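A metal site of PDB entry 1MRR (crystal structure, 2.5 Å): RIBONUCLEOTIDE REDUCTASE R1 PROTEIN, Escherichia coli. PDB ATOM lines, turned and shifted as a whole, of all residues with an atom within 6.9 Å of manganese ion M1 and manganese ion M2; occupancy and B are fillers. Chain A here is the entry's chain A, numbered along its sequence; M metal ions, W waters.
O of Asp 237 sits close to NE2 of His 241 (3.4 Å). NE1 of Trp 111 lies close to OE1 of Glu 204 (3.4 Å). A ring nitrogen (NE2) of His 241 sits close to the side-chain hydroxyl (OG) of Ser 114 (3.0 Å). The side-chain hydroxyl (OG) of Ser 114 sits at hydrogen-bond distance from the backbone carbonyl oxygen (O) of Trp 111 (3.1 Å). The side-chain carboxylate of Asp 84 sits at hydrogen-bond distance from the side-chain hydroxyl of Tyr 122, 2.9 Å away. NE2 of His 118 lies close to O of Ser 114, at 3.2 Å. NE1 of Trp 111 lies close to OE2 of Glu 115 (3.3 Å). OG of Ser 119 sits at hydrogen-bond distance from O of Glu 115.
NE1 of Trp 111 touches manganese ion M1, at 3.9 Å. Within 4 Å of manganese ion M1: Trp 111, Glu 115, Glu 204, Glu 238 and His 241. The nearest printed residue that does not touch manganese ion M1 is Gln 87 (4.7 Å).
Four residues have an atom within 4 Å of manganese ion M2: Asp 84, Glu 115, His 118 and Glu 238. The nearest printed residue that does not touch manganese ion M2 is Phe 208 (4.2 Å).
OE1 of Glu 238 is bound to manganese ion M1. The side-chain carboxylate (OE2) of Glu 204 binds manganese ion M1 (1.9 Å). Manganese ion M1 is bound by OE2 of Glu 115, at 2.2 Å. ND1 of His 241 is bound to manganese ion M1, 2.3 Å away. Water W1 is bound to manganese ion M1. Slightly farther from manganese ion M1 lies the side-chain carboxylate (OE2) of Glu 238 (2.9 Å).
OE2 of Glu 238 binds manganese ion M2, at 2.1 Å. Manganese ion M2 is bound by OD1 of Asp 84. Manganese ion M2 is bound by the side-chain carboxylate (OE1) of Glu 115 (2.2 Å). A ring nitrogen (ND1) of His 118 binds manganese ion M2. Slightly farther from manganese ion M2 lies water W1 (2.8 Å). Slightly farther from manganese ion M2 lies OD2 of Asp 84 (2.9 Å).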
ATOM      1  N   GLN A  80     -10.756  25.915 -35.061  1.00  0.00           N
ATOM      2  CA  GLN A  80     -11.771  25.162 -34.341  1.00  0.00           C
ATOM      3  C   GLN A  80     -11.333  23.706 -34.260  1.00  0.00           C
ATOM      4  O   GLN A  80     -11.371  23.115 -33.173  1.00  0.00           O
ATOM      5  CB  GLN A  80     -13.109  25.255 -35.070  1.00  0.00           C
ATOM      6  CG  GLN A  80     -13.717  26.642 -35.052  1.00  0.00           C
ATOM      7  CD  GLN A  80     -14.984  26.835 -35.868  1.00  0.00           C
ATOM      8  OE1 GLN A  80     -15.241  26.202 -36.893  1.00  0.00           O
ATOM      9  NE2 GLN A  80     -15.841  27.770 -35.496  1.00  0.00           N
ATOM     10  N   LEU A  83      -8.569  23.308 -31.564  1.00  0.00           N
ATOM     11  CA  LEU A  83      -9.060  23.354 -30.212  1.00  0.00           C
ATOM     12  C   LEU A  83      -9.824  22.076 -29.856  1.00  0.00           C
ATOM     13  O   LEU A  83      -9.513  21.474 -28.823  1.00  0.00           O
ATOM     14  CB  LEU A  83      -9.947  24.616 -30.016  1.00  0.00           C
ATOM     15  CG  LEU A  83      -9.266  26.004 -30.082  1.00  0.00           C
ATOM     16  CD1 LEU A  83     -10.261  27.085 -29.684  1.00  0.00           C
ATOM     17  CD2 LEU A  83      -8.080  26.059 -29.146  1.00  0.00           C
ATOM     18  N   ASP A  84     -10.785  21.565 -30.681  1.00  0.00           N
ATOM     19  CA  ASP A  84     -11.453  20.339 -30.294  1.00  0.00           C
ATOM     20  C   ASP A  84     -10.587  19.104 -30.332  1.00  0.00           C
ATOM     21  O   ASP A  84     -10.828  18.177 -29.543  1.00  0.00           O
ATOM     22  CB  ASP A  84     -12.646  20.122 -31.131  1.00  0.00           C
ATOM     23  CG  ASP A  84     -13.848  20.867 -30.564  1.00  0.00           C
ATOM     24  OD1 ASP A  84     -14.046  20.883 -29.339  1.00  0.00           O
ATOM     25  OD2 ASP A  84     -14.617  21.417 -31.360  1.00  0.00           O
ATOM     26  N   GLN A  87      -9.274  19.336 -26.863  1.00  0.00           N
ATOM     27  CA  GLN A  87     -10.330  19.175 -25.869  1.00  0.00           C
ATOM     28  C   GLN A  87     -10.906  17.770 -25.874  1.00  0.00           C
ATOM     29  O   GLN A  87     -11.566  17.393 -24.917  1.00  0.00           O
ATOM     30  CB  GLN A  87     -11.462  20.178 -26.120  1.00  0.00           C
ATOM     31  CG  GLN A  87     -11.011  21.572 -25.701  1.00  0.00           C
ATOM     32  CD  GLN A  87     -10.761  21.680 -24.204  1.00  0.00           C
ATOM     33  OE1 GLN A  87      -9.625  21.627 -23.748  1.00  0.00           O
ATOM     34  NE2 GLN A  87     -11.823  21.786 -23.392  1.00  0.00           N
ATOM     35  N   TRP A 111     -17.995  15.176 -21.286  1.00  0.00           N
ATOM     36  CA  TRP A 111     -17.511  16.420 -21.850  1.00  0.00           C
ATOM     37  C   TRP A 111     -16.430  16.104 -22.896  1.00  0.00           C
ATOM     38  O   TRP A 111     -16.536  16.627 -24.012  1.00  0.00           O
ATOM     39  CB  TRP A 111     -17.002  17.267 -20.662  1.00  0.00           C
ATOM     40  CG  TRP A 111     -16.193  18.526 -20.949  1.00  0.00           C
ATOM     41  CD1 TRP A 111     -16.188  19.169 -22.164  1.00  0.00           C
ATOM     42  CD2 TRP A 111     -15.368  19.127 -20.047  1.00  0.00           C
ATOM     43  NE1 TRP A 111     -15.362  20.171 -22.032  1.00  0.00           N
ATOM     44  CE2 TRP A 111     -14.859  20.186 -20.782  1.00  0.00           C
ATOM     45  CE3 TRP A 111     -15.004  18.928 -18.715  1.00  0.00           C
ATOM     46  CZ2 TRP A 111     -13.958  21.060 -20.199  1.00  0.00           C
ATOM     47  CZ3 TRP A 111     -14.113  19.804 -18.134  1.00  0.00           C
ATOM     48  CH2 TRP A 111     -13.595  20.851 -18.877  1.00  0.00           C
ATOM     49  N   SER A 114     -18.235  14.544 -26.067  1.00  0.00           N
ATOM     50  CA  SER A 114     -18.889  15.448 -27.021  1.00  0.00           C
ATOM     51  C   SER A 114     -17.898  16.281 -27.868  1.00  0.00           C
ATOM     52  O   SER A 114     -18.238  16.759 -28.959  1.00  0.00           O
ATOM     53  CB  SER A 114     -19.835  16.360 -26.229  1.00  0.00           C
ATOM     54  OG  SER A 114     -19.216  17.370 -25.445  1.00  0.00           O
ATOM     55  N   GLU A 115     -16.645  16.454 -27.418  1.00  0.00           N
ATOM     56  CA  GLU A 115     -15.636  17.128 -28.181  1.00  0.00           C
ATOM     57  C   GLU A 115     -15.221  16.228 -29.312  1.00  0.00           C
ATOM     58  O   GLU A 115     -15.041  16.755 -30.412  1.00  0.00           O
ATOM     59  CB  GLU A 115     -14.421  17.453 -27.329  1.00  0.00           C
ATOM     60  CG  GLU A 115     -14.700  18.312 -26.080  1.00  0.00           C
ATOM     61  CD  GLU A 115     -15.257  19.735 -26.215  1.00  0.00           C
ATOM     62  OE1 GLU A 115     -15.924  20.089 -27.207  1.00  0.00           O
ATOM     63  OE2 GLU A 115     -15.011  20.483 -25.272  1.00  0.00           O
ATOM     64  N   THR A 116     -15.169  14.900 -29.173  1.00  0.00           N
ATOM     65  CA  THR A 116     -14.754  14.073 -30.293  1.00  0.00           C
ATOM     66  C   THR A 116     -15.849  14.106 -31.383  1.00  0.00           C
ATOM     67  O   THR A 116     -15.579  13.992 -32.595  1.00  0.00           O
ATOM     68  CB  THR A 116     -14.425  12.608 -29.766  1.00  0.00           C
ATOM     69  OG1 THR A 116     -15.569  11.982 -29.221  1.00  0.00           O
ATOM     70  CG2 THR A 116     -13.380  12.663 -28.654  1.00  0.00           C
ATOM     71  N   HIS A 118     -17.461  16.836 -32.097  1.00  0.00           N
ATOM     72  CA  HIS A 118     -17.182  18.138 -32.722  1.00  0.00           C
ATOM     73  C   HIS A 118     -16.055  17.898 -33.707  1.00  0.00           C
ATOM     74  O   HIS A 118     -16.164  18.349 -34.824  1.00  0.00           O
ATOM     75  CB  HIS A 118     -16.765  19.159 -31.651  1.00  0.00           C
ATOM     76  CG  HIS A 118     -17.855  19.479 -30.608  1.00  0.00           C
ATOM     77  ND1 HIS A 118     -17.755  20.208 -29.500  1.00  0.00           N
ATOM     78  CD2 HIS A 118     -19.166  19.045 -30.706  1.00  0.00           C
ATOM     79  CE1 HIS A 118     -18.936  20.223 -28.947  1.00  0.00           C
ATOM     80  NE2 HIS A 118     -19.772  19.529 -29.678  1.00  0.00           N
ATOM     81  N   SER A 119     -14.981  17.219 -33.331  1.00  0.00           N
ATOM     82  CA  SER A 119     -13.944  16.826 -34.273  1.00  0.00           C
ATOM     83  C   SER A 119     -14.530  16.110 -35.506  1.00  0.00           C
ATOM     84  O   SER A 119     -14.239  16.500 -36.637  1.00  0.00           O
ATOM     85  CB  SER A 119     -12.933  15.913 -33.576  1.00  0.00           C
ATOM     86  OG  SER A 119     -12.321  16.611 -32.511  1.00  0.00           O
ATOM     87  N   TYR A 122     -16.103  18.442 -37.990  1.00  0.00           N
ATOM     88  CA  TYR A 122     -15.145  19.166 -38.794  1.00  0.00           C
ATOM     89  C   TYR A 122     -14.673  18.292 -39.954  1.00  0.00           C
ATOM     90  O   TYR A 122     -14.650  18.767 -41.106  1.00  0.00           O
ATOM     91  CB  TYR A 122     -13.981  19.610 -37.919  1.00  0.00           C
ATOM     92  CG  TYR A 122     -14.431  20.575 -36.825  1.00  0.00           C
ATOM     93  CD1 TYR A 122     -15.417  21.529 -37.028  1.00  0.00           C
ATOM     94  CD2 TYR A 122     -13.842  20.459 -35.580  1.00  0.00           C
ATOM     95  CE1 TYR A 122     -15.812  22.344 -35.976  1.00  0.00           C
ATOM     96  CE2 TYR A 122     -14.237  21.274 -34.528  1.00  0.00           C
ATOM     97  CZ  TYR A 122     -15.220  22.206 -34.730  1.00  0.00           C
ATOM     98  OH  TYR A 122     -15.636  22.950 -33.632  1.00  0.00           O
ATOM     99  N   LEU A 203     -10.722  29.222 -22.924  1.00  0.00           N
ATOM    100  CA  LEU A 203     -10.821  28.526 -24.204  1.00  0.00           C
ATOM    101  C   LEU A 203     -12.243  28.300 -24.648  1.00  0.00           C
ATOM    102  O   LEU A 203     -12.603  28.703 -25.763  1.00  0.00           O
ATOM    103  CB  LEU A 203      -9.998  27.198 -24.068  1.00  0.00           C
ATOM    104  CG  LEU A 203     -10.213  25.825 -24.787  1.00  0.00           C
ATOM    105  CD1 LEU A 203     -10.622  26.034 -26.199  1.00  0.00           C
ATOM    106  CD2 LEU A 203      -8.911  25.020 -24.806  1.00  0.00           C
ATOM    107  N   GLU A 204     -13.087  27.735 -23.779  1.00  0.00           N
ATOM    108  CA  GLU A 204     -14.457  27.427 -24.183  1.00  0.00           C
ATOM    109  C   GLU A 204     -15.413  28.601 -24.225  1.00  0.00           C
ATOM    110  O   GLU A 204     -16.363  28.662 -25.021  1.00  0.00           O
ATOM    111  CB  GLU A 204     -15.046  26.359 -23.270  1.00  0.00           C
ATOM    112  CG  GLU A 204     -14.115  25.175 -23.284  1.00  0.00           C
ATOM    113  CD  GLU A 204     -14.780  23.843 -23.041  1.00  0.00           C
ATOM    114  OE1 GLU A 204     -15.231  23.600 -21.940  1.00  0.00           O
ATOM    115  OE2 GLU A 204     -14.836  23.033 -23.957  1.00  0.00           O
ATOM    116  N   PHE A 208     -13.856  29.920 -28.471  1.00  0.00           N
ATOM    117  CA  PHE A 208     -14.787  29.290 -29.374  1.00  0.00           C
ATOM    118  C   PHE A 208     -15.809  30.292 -29.807  1.00  0.00           C
ATOM    119  O   PHE A 208     -16.215  30.293 -30.977  1.00  0.00           O
ATOM    120  CB  PHE A 208     -15.488  28.086 -28.719  1.00  0.00           C
ATOM    121  CG  PHE A 208     -14.859  26.792 -29.241  1.00  0.00           C
ATOM    122  CD1 PHE A 208     -14.989  26.457 -30.585  1.00  0.00           C
ATOM    123  CD2 PHE A 208     -14.084  25.986 -28.415  1.00  0.00           C
ATOM    124  CE1 PHE A 208     -14.351  25.350 -31.114  1.00  0.00           C
ATOM    125  CE2 PHE A 208     -13.444  24.879 -28.954  1.00  0.00           C
ATOM    126  CZ  PHE A 208     -13.589  24.568 -30.290  1.00  0.00           C
ATOM    127  N   PHE A 212     -17.129  31.191 -33.490  1.00  0.00           N
ATOM    128  CA  PHE A 212     -18.528  31.024 -33.837  1.00  0.00           C
ATOM    129  C   PHE A 212     -19.041  32.267 -34.566  1.00  0.00           C
ATOM    130  O   PHE A 212     -19.747  32.139 -35.561  1.00  0.00           O
ATOM    131  CB  PHE A 212     -19.375  30.810 -32.578  1.00  0.00           C
ATOM    132  CG  PHE A 212     -19.141  29.536 -31.792  1.00  0.00           C
ATOM    133  CD1 PHE A 212     -18.471  28.451 -32.335  1.00  0.00           C
ATOM    134  CD2 PHE A 212     -19.614  29.475 -30.489  1.00  0.00           C
ATOM    135  CE1 PHE A 212     -18.261  27.312 -31.582  1.00  0.00           C
ATOM    136  CE2 PHE A 212     -19.416  28.329 -29.739  1.00  0.00           C
ATOM    137  CZ  PHE A 212     -18.737  27.242 -30.280  1.00  0.00           C
ATOM    138  N   ILE A 234     -22.767  22.680 -32.105  1.00  0.00           N
ATOM    139  CA  ILE A 234     -21.537  22.733 -31.344  1.00  0.00           C
ATOM    140  C   ILE A 234     -21.638  23.780 -30.262  1.00  0.00           C
ATOM    141  O   ILE A 234     -21.290  23.493 -29.107  1.00  0.00           O
ATOM    142  CB  ILE A 234     -20.364  23.044 -32.304  1.00  0.00           C
ATOM    143  CG1 ILE A 234     -20.149  21.776 -33.131  1.00  0.00           C
ATOM    144  CG2 ILE A 234     -19.085  23.471 -31.550  1.00  0.00           C
ATOM    145  CD1 ILE A 234     -18.910  21.853 -34.050  1.00  0.00           C
ATOM    146  N   ASP A 237     -23.465  22.862 -27.216  1.00  0.00           N
ATOM    147  CA  ASP A 237     -22.745  22.003 -26.299  1.00  0.00           C
ATOM    148  C   ASP A 237     -21.706  22.855 -25.578  1.00  0.00           C
ATOM    149  O   ASP A 237     -21.464  22.671 -24.371  1.00  0.00           O
ATOM    150  CB  ASP A 237     -22.028  20.895 -27.017  1.00  0.00           C
ATOM    151  CG  ASP A 237     -22.876  19.821 -27.663  1.00  0.00           C
ATOM    152  OD1 ASP A 237     -24.015  19.541 -27.277  1.00  0.00           O
ATOM    153  OD2 ASP A 237     -22.366  19.234 -28.588  1.00  0.00           O
ATOM    154  N   GLU A 238     -21.028  23.783 -26.250  1.00  0.00           N
ATOM    155  CA  GLU A 238     -20.073  24.631 -25.545  1.00  0.00           C
ATOM    156  C   GLU A 238     -20.704  25.429 -24.407  1.00  0.00           C
ATOM    157  O   GLU A 238     -20.005  25.633 -23.412  1.00  0.00           O
ATOM    158  CB  GLU A 238     -19.373  25.602 -26.478  1.00  0.00           C
ATOM    159  CG  GLU A 238     -18.510  24.901 -27.489  1.00  0.00           C
ATOM    160  CD  GLU A 238     -17.548  23.808 -27.007  1.00  0.00           C
ATOM    161  OE1 GLU A 238     -16.959  23.924 -25.922  1.00  0.00           O
ATOM    162  OE2 GLU A 238     -17.354  22.846 -27.763  1.00  0.00           O
ATOM    163  N   ALA A 239     -21.985  25.806 -24.501  1.00  0.00           N
ATOM    164  CA  ALA A 239     -22.717  26.452 -23.434  1.00  0.00           C
ATOM    165  C   ALA A 239     -22.612  25.624 -22.159  1.00  0.00           C
ATOM    166  O   ALA A 239     -22.254  26.107 -21.085  1.00  0.00           O
ATOM    167  CB  ALA A 239     -24.209  26.553 -23.735  1.00  0.00           C
ATOM    168  N   HIS A 241     -20.401  23.215 -21.518  1.00  0.00           N
ATOM    169  CA  HIS A 241     -19.022  22.973 -21.088  1.00  0.00           C
ATOM    170  C   HIS A 241     -18.498  24.114 -20.260  1.00  0.00           C
ATOM    171  O   HIS A 241     -17.916  23.898 -19.201  1.00  0.00           O
ATOM    172  CB  HIS A 241     -18.161  22.769 -22.297  1.00  0.00           C
ATOM    173  CG  HIS A 241     -18.550  21.579 -23.191  1.00  0.00           C
ATOM    174  ND1 HIS A 241     -17.901  21.137 -24.261  1.00  0.00           N
ATOM    175  CD2 HIS A 241     -19.646  20.763 -22.996  1.00  0.00           C
ATOM    176  CE1 HIS A 241     -18.572  20.098 -24.709  1.00  0.00           C
ATOM    177  NE2 HIS A 241     -19.608  19.895 -23.946  1.00  0.00           N
ATOM    178  N   LEU A 242     -18.837  25.325 -20.721  1.00  0.00           N
ATOM    179  CA  LEU A 242     -18.568  26.614 -20.094  1.00  0.00           C
ATOM    180  C   LEU A 242     -19.250  26.676 -18.719  1.00  0.00           C
ATOM    181  O   LEU A 242     -18.615  26.960 -17.695  1.00  0.00           O
ATOM    182  CB  LEU A 242     -19.114  27.643 -21.066  1.00  0.00           C
ATOM    183  CG  LEU A 242     -19.418  29.137 -20.947  1.00  0.00           C
ATOM    184  CD1 LEU A 242     -19.739  29.571 -22.381  1.00  0.00           C
ATOM    185  CD2 LEU A 242     -20.651  29.475 -20.135  1.00  0.00           C
HETATM  186 MN    MN M   1     -16.156  22.328 -25.191  1.00  0.00          MN
HETATM  187 MN    MN M   2     -16.069  21.565 -28.840  1.00  0.00          MN
HETATM  188  O   HOH W   1     -14.367  22.713 -26.946  1.00  0.00           O
